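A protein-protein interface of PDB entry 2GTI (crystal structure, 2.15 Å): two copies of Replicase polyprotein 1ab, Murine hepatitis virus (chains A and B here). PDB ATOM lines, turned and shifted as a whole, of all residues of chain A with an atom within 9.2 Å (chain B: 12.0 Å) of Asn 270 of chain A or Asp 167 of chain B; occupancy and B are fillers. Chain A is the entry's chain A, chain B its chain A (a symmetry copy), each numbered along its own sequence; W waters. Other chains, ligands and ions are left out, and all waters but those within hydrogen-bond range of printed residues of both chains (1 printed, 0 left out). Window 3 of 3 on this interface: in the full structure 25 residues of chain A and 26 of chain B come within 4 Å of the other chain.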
ATOM      1  N   GLY A 267      37.973   4.785 -19.843  1.00  0.00           N
ATOM      2  CA  GLY A 267      37.121   3.609 -19.846  1.00  0.00           C
ATOM      3  C   GLY A 267      35.693   3.936 -20.255  1.00  0.00           C
ATOM      4  O   GLY A 267      35.194   5.024 -19.960  1.00  0.00           O
ATOM      5  N   SER A 268      35.042   3.006 -20.950  1.00  0.00           N
ATOM      6  CA  SER A 268      33.652   3.192 -21.376  1.00  0.00           C
ATOM      7  C   SER A 268      32.780   2.201 -20.608  1.00  0.00           C
ATOM      8  O   SER A 268      33.098   1.015 -20.519  1.00  0.00           O
ATOM      9  CB  SER A 268      33.507   2.957 -22.883  1.00  0.00           C
ATOM     10  OG  SER A 268      33.852   1.630 -23.231  1.00  0.00           O
ATOM     11  N   PHE A 269      31.676   2.689 -20.059  1.00  0.00           N
ATOM     12  CA  PHE A 269      30.788   1.846 -19.272  1.00  0.00           C
ATOM     13  C   PHE A 269      29.385   1.713 -19.862  1.00  0.00           C
ATOM     14  O   PHE A 269      28.426   1.452 -19.137  1.00  0.00           O
ATOM     15  CB  PHE A 269      30.712   2.415 -17.854  1.00  0.00           C
ATOM     16  CG  PHE A 269      32.059   2.560 -17.191  1.00  0.00           C
ATOM     17  CD1 PHE A 269      32.618   1.504 -16.476  1.00  0.00           C
ATOM     18  CD2 PHE A 269      32.784   3.741 -17.314  1.00  0.00           C
ATOM     19  CE1 PHE A 269      33.883   1.621 -15.894  1.00  0.00           C
ATOM     20  CE2 PHE A 269      34.050   3.870 -16.738  1.00  0.00           C
ATOM     21  CZ  PHE A 269      34.602   2.808 -16.026  1.00  0.00           C
ATOM     22  N   ASN A 270      29.270   1.873 -21.177  1.00  0.00           N
ATOM     23  CA  ASN A 270      27.976   1.783 -21.851  1.00  0.00           C
ATOM     24  C   ASN A 270      27.698   0.456 -22.543  1.00  0.00           C
ATOM     25  O   ASN A 270      26.922   0.406 -23.493  1.00  0.00           O
ATOM     26  CB  ASN A 270      27.838   2.912 -22.871  1.00  0.00           C
ATOM     27  CG  ASN A 270      27.623   4.256 -22.220  1.00  0.00           C
ATOM     28  OD1 ASN A 270      27.548   5.284 -22.897  1.00  0.00           O
ATOM     29  ND2 ASN A 270      27.514   4.259 -20.894  1.00  0.00           N
ATOM     30  N   GLN A 271      28.328  -0.614 -22.074  1.00  0.00           N
ATOM     31  CA  GLN A 271      28.118  -1.934 -22.658  1.00  0.00           C
ATOM     32  C   GLN A 271      28.259  -2.958 -21.550  1.00  0.00           C
ATOM     33  O   GLN A 271      28.677  -2.623 -20.449  1.00  0.00           O
ATOM     34  CB  GLN A 271      29.161  -2.240 -23.739  1.00  0.00           C
ATOM     35  CG  GLN A 271      29.521  -1.068 -24.618  1.00  0.00           C
ATOM     36  CD  GLN A 271      30.545  -0.150 -23.973  1.00  0.00           C
ATOM     37  OE1 GLN A 271      30.797   0.950 -24.461  1.00  0.00           O
ATOM     38  NE2 GLN A 271      31.148  -0.605 -22.875  1.00  0.00           N
ATOM     39  N   LYS A 272      27.914  -4.205 -21.847  1.00  0.00           N
ATOM     40  CA  LYS A 272      28.019  -5.265 -20.859  1.00  0.00           C
ATOM     41  C   LYS A 272      29.469  -5.379 -20.411  1.00  0.00           C
ATOM     42  O   LYS A 272      29.754  -5.498 -19.224  1.00  0.00           O
ATOM     43  CB  LYS A 272      27.550  -6.598 -21.451  1.00  0.00           C
ATOM     44  CG  LYS A 272      26.068  -6.646 -21.787  1.00  0.00           C
ATOM     45  CD  LYS A 272      25.677  -7.975 -22.424  1.00  0.00           C
ATOM     46  CE  LYS A 272      25.949  -9.149 -21.493  1.00  0.00           C
ATOM     47  NZ  LYS A 272      25.500 -10.460 -22.063  1.00  0.00           N
ATOM     48  N   ILE A 273      30.379  -5.333 -21.376  1.00  0.00           N
ATOM     49  CA  ILE A 273      31.803  -5.446 -21.085  1.00  0.00           C
ATOM     50  C   ILE A 273      32.486  -4.085 -21.086  1.00  0.00           C
ATOM     51  O   ILE A 273      32.448  -3.353 -22.080  1.00  0.00           O
ATOM     52  CB  ILE A 273      32.504  -6.351 -22.118  1.00  0.00           C
ATOM     53  CG1 ILE A 273      31.829  -7.724 -22.134  1.00  0.00           C
ATOM     54  CG2 ILE A 273      33.983  -6.486 -21.782  1.00  0.00           C
ATOM     55  CD1 ILE A 273      32.359  -8.653 -23.200  1.00  0.00           C
ATOM     56  N   ILE A 274      33.104  -3.752 -19.959  1.00  0.00           N
ATOM     57  CA  ILE A 274      33.814  -2.492 -19.820  1.00  0.00           C
ATOM     58  C   ILE A 274      34.818  -2.369 -20.958  1.00  0.00           C
ATOM     59  O   ILE A 274      35.361  -3.366 -21.429  1.00  0.00           O
ATOM     60  CB  ILE A 274      34.561  -2.431 -18.471  1.00  0.00           C
ATOM     61  CG1 ILE A 274      33.548  -2.470 -17.319  1.00  0.00           C
ATOM     62  CG2 ILE A 274      35.417  -1.170 -18.402  1.00  0.00           C
ATOM     63  CD1 ILE A 274      34.178  -2.523 -15.948  1.00  0.00           C
ATOM     64  N   GLY A 275      35.045  -1.144 -21.413  1.00  0.00           N
ATOM     65  CA  GLY A 275      35.995  -0.935 -22.489  1.00  0.00           C
ATOM     66  C   GLY A 275      37.207  -0.195 -21.969  1.00  0.00           C
ATOM     67  O   GLY A 275      37.065   0.777 -21.228  1.00  0.00           O
ATOM     68  N   ARG A 286      37.038   7.138 -11.860  1.00  0.00           N
ATOM     69  CA  ARG A 286      35.698   6.566 -11.932  1.00  0.00           C
ATOM     70  C   ARG A 286      35.119   6.428 -10.527  1.00  0.00           C
ATOM     71  O   ARG A 286      33.932   6.689 -10.298  1.00  0.00           O
ATOM     72  CB  ARG A 286      35.751   5.190 -12.606  1.00  0.00           C
ATOM     73  CG  ARG A 286      34.397   4.479 -12.695  1.00  0.00           C
ATOM     74  CD  ARG A 286      33.436   5.238 -13.591  1.00  0.00           C
ATOM     75  NE  ARG A 286      32.118   4.612 -13.663  1.00  0.00           N
ATOM     76  CZ  ARG A 286      31.116   5.083 -14.398  1.00  0.00           C
ATOM     77  NH1 ARG A 286      31.293   6.181 -15.118  1.00  0.00           N
ATOM     78  NH2 ARG A 286      29.940   4.466 -14.409  1.00  0.00           N
ATOM     79  N   SER A 290      31.328   6.541  -9.201  1.00  0.00           N
ATOM     80  CA  SER A 290      30.757   5.200  -9.254  1.00  0.00           C
ATOM     81  C   SER A 290      31.644   4.186  -8.549  1.00  0.00           C
ATOM     82  O   SER A 290      32.858   4.157  -8.744  1.00  0.00           O
ATOM     83  CB  SER A 290      30.544   4.776 -10.710  1.00  0.00           C
ATOM     84  OG  SER A 290      30.028   3.461 -10.787  1.00  0.00           O
ATOM     85  N   ASP A 311      31.558  -2.311 -12.411  1.00  0.00           N
ATOM     86  CA  ASP A 311      31.198  -0.913 -12.171  1.00  0.00           C
ATOM     87  C   ASP A 311      29.759  -0.874 -11.657  1.00  0.00           C
ATOM     88  O   ASP A 311      28.835  -1.315 -12.340  1.00  0.00           O
ATOM     89  CB  ASP A 311      31.297  -0.102 -13.463  1.00  0.00           C
ATOM     90  CG  ASP A 311      30.930   1.355 -13.262  1.00  0.00           C
ATOM     91  OD1 ASP A 311      31.717   2.087 -12.621  1.00  0.00           O
ATOM     92  OD2 ASP A 311      29.848   1.767 -13.738  1.00  0.00           O
ATOM     93  N   GLU A 312      29.571  -0.337 -10.459  1.00  0.00           N
ATOM     94  CA  GLU A 312      28.253  -0.286  -9.843  1.00  0.00           C
ATOM     95  C   GLU A 312      27.176   0.505 -10.588  1.00  0.00           C
ATOM     96  O   GLU A 312      26.127  -0.040 -10.917  1.00  0.00           O
ATOM     97  CB  GLU A 312      28.390   0.235  -8.412  1.00  0.00           C
ATOM     98  CG  GLU A 312      27.114   0.186  -7.596  1.00  0.00           C
ATOM     99  CD  GLU A 312      27.383   0.353  -6.112  1.00  0.00           C
ATOM    100  OE1 GLU A 312      27.910  -0.592  -5.494  1.00  0.00           O
ATOM    101  OE2 GLU A 312      27.083   1.434  -5.566  1.00  0.00           O
ATOM    102  N   ASN A 313      27.431   1.781 -10.854  1.00  0.00           N
ATOM    103  CA  ASN A 313      26.458   2.626 -11.541  1.00  0.00           C
ATOM    104  C   ASN A 313      25.930   2.085 -12.866  1.00  0.00           C
ATOM    105  O   ASN A 313      24.729   2.128 -13.120  1.00  0.00           O
ATOM    106  CB  ASN A 313      27.046   4.019 -11.777  1.00  0.00           C
ATOM    107  CG  ASN A 313      27.125   4.841 -10.508  1.00  0.00           C
ATOM    108  OD1 ASN A 313      26.854   4.347  -9.415  1.00  0.00           O
ATOM    109  ND2 ASN A 313      27.500   6.106 -10.649  1.00  0.00           N
ATOM    110  N   SER A 314      26.818   1.567 -13.703  1.00  0.00           N
ATOM    111  CA  SER A 314      26.408   1.062 -15.007  1.00  0.00           C
ATOM    112  C   SER A 314      26.110  -0.431 -15.063  1.00  0.00           C
ATOM    113  O   SER A 314      25.415  -0.886 -15.969  1.00  0.00           O
ATOM    114  CB  SER A 314      27.483   1.369 -16.043  1.00  0.00           C
ATOM    115  OG  SER A 314      28.611   0.535 -15.834  1.00  0.00           O
ATOM    116  N   GLY A 315      26.635  -1.199 -14.115  1.00  0.00           N
ATOM    117  CA  GLY A 315      26.400  -2.633 -14.150  1.00  0.00           C
ATOM    118  C   GLY A 315      27.226  -3.286 -15.248  1.00  0.00           C
ATOM    119  O   GLY A 315      26.922  -4.378 -15.721  1.00  0.00           O
ATOM    120  N   SER A 316      28.275  -2.597 -15.671  1.00  0.00           N
ATOM    121  CA  SER A 316      29.169  -3.109 -16.701  1.00  0.00           C
ATOM    122  C   SER A 316      30.302  -3.849 -15.983  1.00  0.00           C
ATOM    123  O   SER A 316      30.540  -3.610 -14.800  1.00  0.00           O
ATOM    124  CB  SER A 316      29.735  -1.940 -17.515  1.00  0.00           C
ATOM    125  OG  SER A 316      30.595  -2.396 -18.543  1.00  0.00           O
ATOM    126  N   SER A 317      30.994  -4.740 -16.686  1.00  0.00           N
ATOM    127  CA  SER A 317      32.096  -5.490 -16.080  1.00  0.00           C
ATOM    128  C   SER A 317      33.006  -6.171 -17.115  1.00  0.00           C
ATOM    129  O   SER A 317      32.638  -6.308 -18.284  1.00  0.00           O
ATOM    130  CB  SER A 317      31.540  -6.542 -15.109  1.00  0.00           C
ATOM    131  OG  SER A 317      30.819  -7.559 -15.787  1.00  0.00           O
ATOM    132  N   PRO B  66      24.940 -11.159 -14.700  1.00  0.00           N
ATOM    133  CA  PRO B  66      23.964 -10.604 -13.754  1.00  0.00           C
ATOM    134  C   PRO B  66      22.770 -11.535 -13.565  1.00  0.00           C
ATOM    135  O   PRO B  66      22.296 -12.145 -14.529  1.00  0.00           O
ATOM    136  CB  PRO B  66      23.533  -9.287 -14.411  1.00  0.00           C
ATOM    137  CG  PRO B  66      24.583  -9.019 -15.459  1.00  0.00           C
ATOM    138  CD  PRO B  66      24.951 -10.386 -15.951  1.00  0.00           C
ATOM    139  N   GLN B 153      13.865  -4.142 -10.557  1.00  0.00           N
ATOM    140  CA  GLN B 153      14.935  -3.741 -11.448  1.00  0.00           C
ATOM    141  C   GLN B 153      16.305  -3.590 -10.778  1.00  0.00           C
ATOM    142  O   GLN B 153      16.850  -2.505 -10.661  1.00  0.00           O
ATOM    143  CB  GLN B 153      14.547  -2.455 -12.188  1.00  0.00           C
ATOM    144  CG  GLN B 153      13.276  -2.616 -13.028  1.00  0.00           C
ATOM    145  CD  GLN B 153      13.135  -1.564 -14.119  1.00  0.00           C
ATOM    146  OE1 GLN B 153      13.296  -0.369 -13.872  1.00  0.00           O
ATOM    147  NE2 GLN B 153      12.824  -2.009 -15.333  1.00  0.00           N
ATOM    148  N   ARG B 154      16.845  -4.707 -10.322  1.00  0.00           N
ATOM    149  CA  ARG B 154      18.168  -4.733  -9.728  1.00  0.00           C
ATOM    150  C   ARG B 154      18.639  -6.173  -9.761  1.00  0.00           C
ATOM    151  O   ARG B 154      17.843  -7.108  -9.650  1.00  0.00           O
ATOM    152  CB  ARG B 154      18.187  -4.173  -8.299  1.00  0.00           C
ATOM    153  CG  ARG B 154      16.934  -4.370  -7.490  1.00  0.00           C
ATOM    154  CD  ARG B 154      17.046  -3.605  -6.168  1.00  0.00           C
ATOM    155  NE  ARG B 154      15.746  -3.478  -5.526  1.00  0.00           N
ATOM    156  CZ  ARG B 154      14.819  -2.597  -5.879  1.00  0.00           C
ATOM    157  NH1 ARG B 154      15.045  -1.742  -6.864  1.00  0.00           N
ATOM    158  NH2 ARG B 154      13.649  -2.600  -5.265  1.00  0.00           N
ATOM    159  N   ALA B 155      19.943  -6.332  -9.931  1.00  0.00           N
ATOM    160  CA  ALA B 155      20.549  -7.639 -10.040  1.00  0.00           C
ATOM    161  C   ALA B 155      21.822  -7.742  -9.222  1.00  0.00           C
ATOM    162  O   ALA B 155      22.398  -6.732  -8.806  1.00  0.00           O
ATOM    163  CB  ALA B 155      20.864  -7.906 -11.498  1.00  0.00           C
ATOM    164  N   LEU B 157      25.518  -8.779  -9.517  1.00  0.00           N
ATOM    165  CA  LEU B 157      26.560  -8.954 -10.537  1.00  0.00           C
ATOM    166  C   LEU B 157      27.890  -9.033  -9.803  1.00  0.00           C
ATOM    167  O   LEU B 157      28.421  -8.011  -9.350  1.00  0.00           O
ATOM    168  CB  LEU B 157      26.592  -7.778 -11.526  1.00  0.00           C
ATOM    169  CG  LEU B 157      27.736  -7.775 -12.563  1.00  0.00           C
ATOM    170  CD1 LEU B 157      27.710  -9.050 -13.409  1.00  0.00           C
ATOM    171  CD2 LEU B 157      27.597  -6.549 -13.464  1.00  0.00           C
ATOM    172  N   VAL B 161      25.322  -5.079  -6.158  1.00  0.00           N
ATOM    173  CA  VAL B 161      23.920  -4.820  -6.459  1.00  0.00           C
ATOM    174  C   VAL B 161      23.885  -3.686  -7.454  1.00  0.00           C
ATOM    175  O   VAL B 161      24.309  -2.575  -7.142  1.00  0.00           O
ATOM    176  CB  VAL B 161      23.139  -4.404  -5.194  1.00  0.00           C
ATOM    177  CG1 VAL B 161      21.736  -3.943  -5.573  1.00  0.00           C
ATOM    178  CG2 VAL B 161      23.072  -5.572  -4.228  1.00  0.00           C
ATOM    179  N   VAL B 162      23.394  -3.967  -8.656  1.00  0.00           N
ATOM    180  CA  VAL B 162      23.329  -2.961  -9.700  1.00  0.00           C
ATOM    181  C   VAL B 162      21.890  -2.767 -10.185  1.00  0.00           C
ATOM    182  O   VAL B 162      21.080  -3.698 -10.155  1.00  0.00           O
ATOM    183  CB  VAL B 162      24.255  -3.353 -10.882  1.00  0.00           C
ATOM    184  CG1 VAL B 162      25.684  -3.590 -10.364  1.00  0.00           C
ATOM    185  CG2 VAL B 162      23.730  -4.601 -11.586  1.00  0.00           C
ATOM    186  N   GLU B 163      21.582  -1.542 -10.610  1.00  0.00           N
ATOM    187  CA  GLU B 163      20.250  -1.193 -11.099  1.00  0.00           C
ATOM    188  C   GLU B 163      20.257  -1.180 -12.614  1.00  0.00           C
ATOM    189  O   GLU B 163      19.213  -1.172 -13.262  1.00  0.00           O
ATOM    190  CB  GLU B 163      19.838   0.179 -10.578  1.00  0.00           C
ATOM    191  CG  GLU B 163      19.985   0.318  -9.078  1.00  0.00           C
ATOM    192  CD  GLU B 163      18.765   0.927  -8.433  1.00  0.00           C
ATOM    193  OE1 GLU B 163      18.422   2.079  -8.780  1.00  0.00           O
ATOM    194  OE2 GLU B 163      18.148   0.250  -7.582  1.00  0.00           O
ATOM    195  N   LYS B 164      21.454  -1.175 -13.179  1.00  0.00           N
ATOM    196  CA  LYS B 164      21.610  -1.184 -14.620  1.00  0.00           C
ATOM    197  C   LYS B 164      22.643  -2.236 -14.961  1.00  0.00           C
ATOM    198  O   LYS B 164      23.410  -2.671 -14.098  1.00  0.00           O
ATOM    199  CB  LYS B 164      22.098   0.176 -15.131  1.00  0.00           C
ATOM    200  CG  LYS B 164      21.138   1.330 -14.909  1.00  0.00           C
ATOM    201  CD  LYS B 164      21.525   2.524 -15.772  1.00  0.00           C
ATOM    202  CE  LYS B 164      20.548   3.679 -15.605  1.00  0.00           C
ATOM    203  NZ  LYS B 164      20.508   4.155 -14.192  1.00  0.00           N
ATOM    204  N   VAL B 165      22.648  -2.630 -16.227  1.00  0.00           N
ATOM    205  CA  VAL B 165      23.575  -3.612 -16.763  1.00  0.00           C
ATOM    206  C   VAL B 165      23.933  -3.025 -18.113  1.00  0.00           C
ATOM    207  O   VAL B 165      23.052  -2.798 -18.935  1.00  0.00           O
ATOM    208  CB  VAL B 165      22.893  -4.990 -16.969  1.00  0.00           C
ATOM    209  CG1 VAL B 165      23.782  -5.888 -17.812  1.00  0.00           C
ATOM    210  CG2 VAL B 165      22.607  -5.642 -15.622  1.00  0.00           C
ATOM    211  N   GLY B 166      25.212  -2.763 -18.342  1.00  0.00           N
ATOM    212  CA  GLY B 166      25.605  -2.175 -19.609  1.00  0.00           C
ATOM    213  C   GLY B 166      24.957  -0.808 -19.735  1.00  0.00           C
ATOM    214  O   GLY B 166      24.742  -0.298 -20.835  1.00  0.00           O
ATOM    215  N   ASP B 167      24.633  -0.227 -18.585  1.00  0.00           N
ATOM    216  CA  ASP B 167      24.005   1.082 -18.504  1.00  0.00           C
ATOM    217  C   ASP B 167      22.537   1.042 -18.934  1.00  0.00           C
ATOM    218  O   ASP B 167      21.917   2.080 -19.164  1.00  0.00           O
ATOM    219  CB  ASP B 167      24.781   2.090 -19.356  1.00  0.00           C
ATOM    220  CG  ASP B 167      24.860   3.451 -18.704  1.00  0.00           C
ATOM    221  OD1 ASP B 167      25.308   3.524 -17.539  1.00  0.00           O
ATOM    222  OD2 ASP B 167      24.479   4.446 -19.356  1.00  0.00           O
ATOM    223  N   SER B 168      21.990  -0.165 -19.040  1.00  0.00           N
ATOM    224  CA  SER B 168      20.593  -0.351 -19.415  1.00  0.00           C
ATOM    225  C   SER B 168      19.861  -0.899 -18.197  1.00  0.00           C
ATOM    226  O   SER B 168      20.443  -1.648 -17.414  1.00  0.00           O
ATOM    227  CB  SER B 168      20.477  -1.340 -20.573  1.00  0.00           C
ATOM    228  OG  SER B 168      21.167  -0.865 -21.712  1.00  0.00           O
ATOM    229  N   ASP B 169      18.595  -0.527 -18.029  1.00  0.00           N
ATOM    230  CA  ASP B 169      17.841  -1.006 -16.877  1.00  0.00           C
ATOM    231  C   ASP B 169      17.849  -2.525 -16.773  1.00  0.00           C
ATOM    232  O   ASP B 169      17.770  -3.232 -17.777  1.00  0.00           O
ATOM    233  CB  ASP B 169      16.392  -0.520 -16.925  1.00  0.00           C
ATOM    234  CG  ASP B 169      16.281   0.976 -16.758  1.00  0.00           C
ATOM    235  OD1 ASP B 169      16.990   1.528 -15.888  1.00  0.00           O
ATOM    236  OD2 ASP B 169      15.479   1.597 -17.489  1.00  0.00           O
ATOM    237  N   VAL B 170      17.963  -3.015 -15.547  1.00  0.00           N
ATOM    238  CA  VAL B 170      17.958  -4.443 -15.299  1.00  0.00           C
ATOM    239  C   VAL B 170      16.529  -4.932 -15.485  1.00  0.00           C
ATOM    240  O   VAL B 170      15.591  -4.302 -15.012  1.00  0.00           O
ATOM    241  CB  VAL B 170      18.394  -4.766 -13.853  1.00  0.00           C
ATOM    242  CG1 VAL B 170      17.998  -6.199 -13.494  1.00  0.00           C
ATOM    243  CG2 VAL B 170      19.902  -4.572 -13.706  1.00  0.00           C
ATOM    244  N   GLU B 171      16.365  -6.047 -16.184  1.00  0.00           N
ATOM    245  CA  GLU B 171      15.041  -6.620 -16.395  1.00  0.00           C
ATOM    246  C   GLU B 171      15.073  -8.142 -16.248  1.00  0.00           C
ATOM    247  O   GLU B 171      15.840  -8.825 -16.923  1.00  0.00           O
ATOM    248  CB  GLU B 171      14.504  -6.244 -17.782  1.00  0.00           C
ATOM    249  CG  GLU B 171      13.261  -7.029 -18.184  1.00  0.00           C
ATOM    250  CD  GLU B 171      12.636  -6.550 -19.486  1.00  0.00           C
ATOM    251  OE1 GLU B 171      13.383  -6.299 -20.461  1.00  0.00           O
ATOM    252  OE2 GLU B 171      11.392  -6.440 -19.539  1.00  0.00           O
HETATM  253  O   HOH W   1      23.601   0.364 -10.645  1.00  0.00           O
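The backbone carbonyl oxygen (O) of Phe 269 of chain A lies close to the side-chain hydroxyl (OG) of Ser 314 of chain A (3.4 Å).
The side-chain amide nitrogen (NE2) of Gln 271 of chain A lies within hydrogen-bond range of the backbone carbonyl oxygen (O) of Ile 273 of chain A (3.1 Å).
The side-chain hydroxyl (OG) of Ser 316 of chain A lies within hydrogen-bond range of the backbone carbonyl oxygen (O) of Gln 271 of chain A.
OG of Ser 316 of chain A is in hydrogen-bond range of O of Lys 272 of chain A, at 3.3 Å.
The backbone carbonyl oxygen of Lys 272 of chain A sits at hydrogen-bond distance from the backbone NH of Ser 317 of chain A (2.9 Å).
The side-chain hydroxyl (OG) of Ser 290 of chain A lies within hydrogen-bond range of the backbone NH (N) of Asn 313 of chain A (3.1 Å).
No residue of chain B comes within 4 Å of Ser 268 of chain A.
Phe 269 of chain A touches one residue of chain B.
Of chain B, only Gly 166 and Asp 167 come within 4 Å of Asn 270 of chain A.
Of chain B, only Gly 166 (3.2 Å) comes within 4 Å of Gln 271 of chain A.
Ile 273 of chain A touches none of the printed residues of chain B.
Ser 314 of chain A touches just these residues of chain B: Lys 164, Val 165, Gly 166 and Asp 167.
Gly 315 of chain A touches just these residues of chain B: Leu 157, Val 162, Lys 164, Val 165 and Gly 166.
Of the printed residues of chain A, Val 161 of chain B touches Glu 312 (3.96 Å).
Glu 163 of chain B touches none of the printed residues of chain A.
Of the printed residues of chain A, Lys 164 of chain B touches Asn 313 (3.8 Å), Ser 314 (3.2 Å) and Gly 315 (3.0 Å).
Of the printed residues of chain A, Val 165 of chain B touches Ser 314 (3.3 Å) and Gly 315 (3.6 Å).
Of the printed residues of chain A, Gly 166 of chain B touches Asn 270, Gln 271, Lys 272, Ser 314 and Gly 315.
Asp 167 of chain B touches just these residues of chain A: Phe 269 (3.7 Å), Asn 270 (3.4 Å) and Ser 314 (2.8 Å).
Ser 168 of chain B touches none of the printed residues of chain A.
The nearest residue of chain B that does not touch Asn 270 of chain A is Ser 168 of chain B (6.2 Å).
Water W1 lies within hydrogen-bond range of O of Glu 312 of chain A (2.6 Å), N of Glu 163 of chain B (2.8 Å) and O of Asn 313 of chain A (3.2 Å).
OD2 of Asp 167 of chain B lies within hydrogen-bond range of ND2 of Asn 270 of chain A (3.4 Å).
O of Ser 314 of chain A lies within hydrogen-bond range of N of Val 165 of chain B (3.3 Å).
The backbone carbonyl oxygen (O) of Ser 314 of chain A lies within hydrogen-bond range of the backbone NH (N) of Gly 166 of chain B, at 3.0 Å.
The backbone NH (N) of Asp 167 of chain B is in hydrogen-bond range of the backbone carbonyl oxygen (O) of Ser 314 of chain A (2.8 Å).
O of Ser 314 of chain A lies close to O of Lys 164 of chain B, 3.3 Å away.
Among the printed residues, merely in contact across the chains: Phe 269 of chain A with Asp 167 of chain B, Asn 270 of chain A with Gly 166 of chain B, Gln 271 of chain A with Gly 166 of chain B, Lys 272 of chain A with Gly 166 of chain B, Glu 312 of chain A with Val 161 of chain B, Glu 312 of chain A with Val 162 of chain B, Asn 313 of chain A with Lys 164 of chain B, Gly 315 of chain A with Leu 157 of chain B, Gly 315 of chain A with Val 162 of chain B, Gly 315 of chain A with Lys 164 of chain B, Gly 315 of chain A with Val 165 of chain B and Gly 315 of chain A with Gly 166 of chain B.
Printed residues of chain B that touch a printed residue of chain A: Leu 157, Val 161, Val 162, Lys 164, Val 165, Gly 166 and Asp 167.
Hydrophobic or aromatic side chains of chain B that line the printed part of chain A: Leu 157 and Val 162.
Among the printed residues, 17 pairs touch across the chains.
Among the printed residues, no Asp or Glu carboxylate lies within 4 Å of a Lys or Arg side-chain nitrogen of the other chain.
No position is printed for both chains.
Of the 17 pairs that touch across the chains among the printed residues, none has its exchanged pair printed and touching as well.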
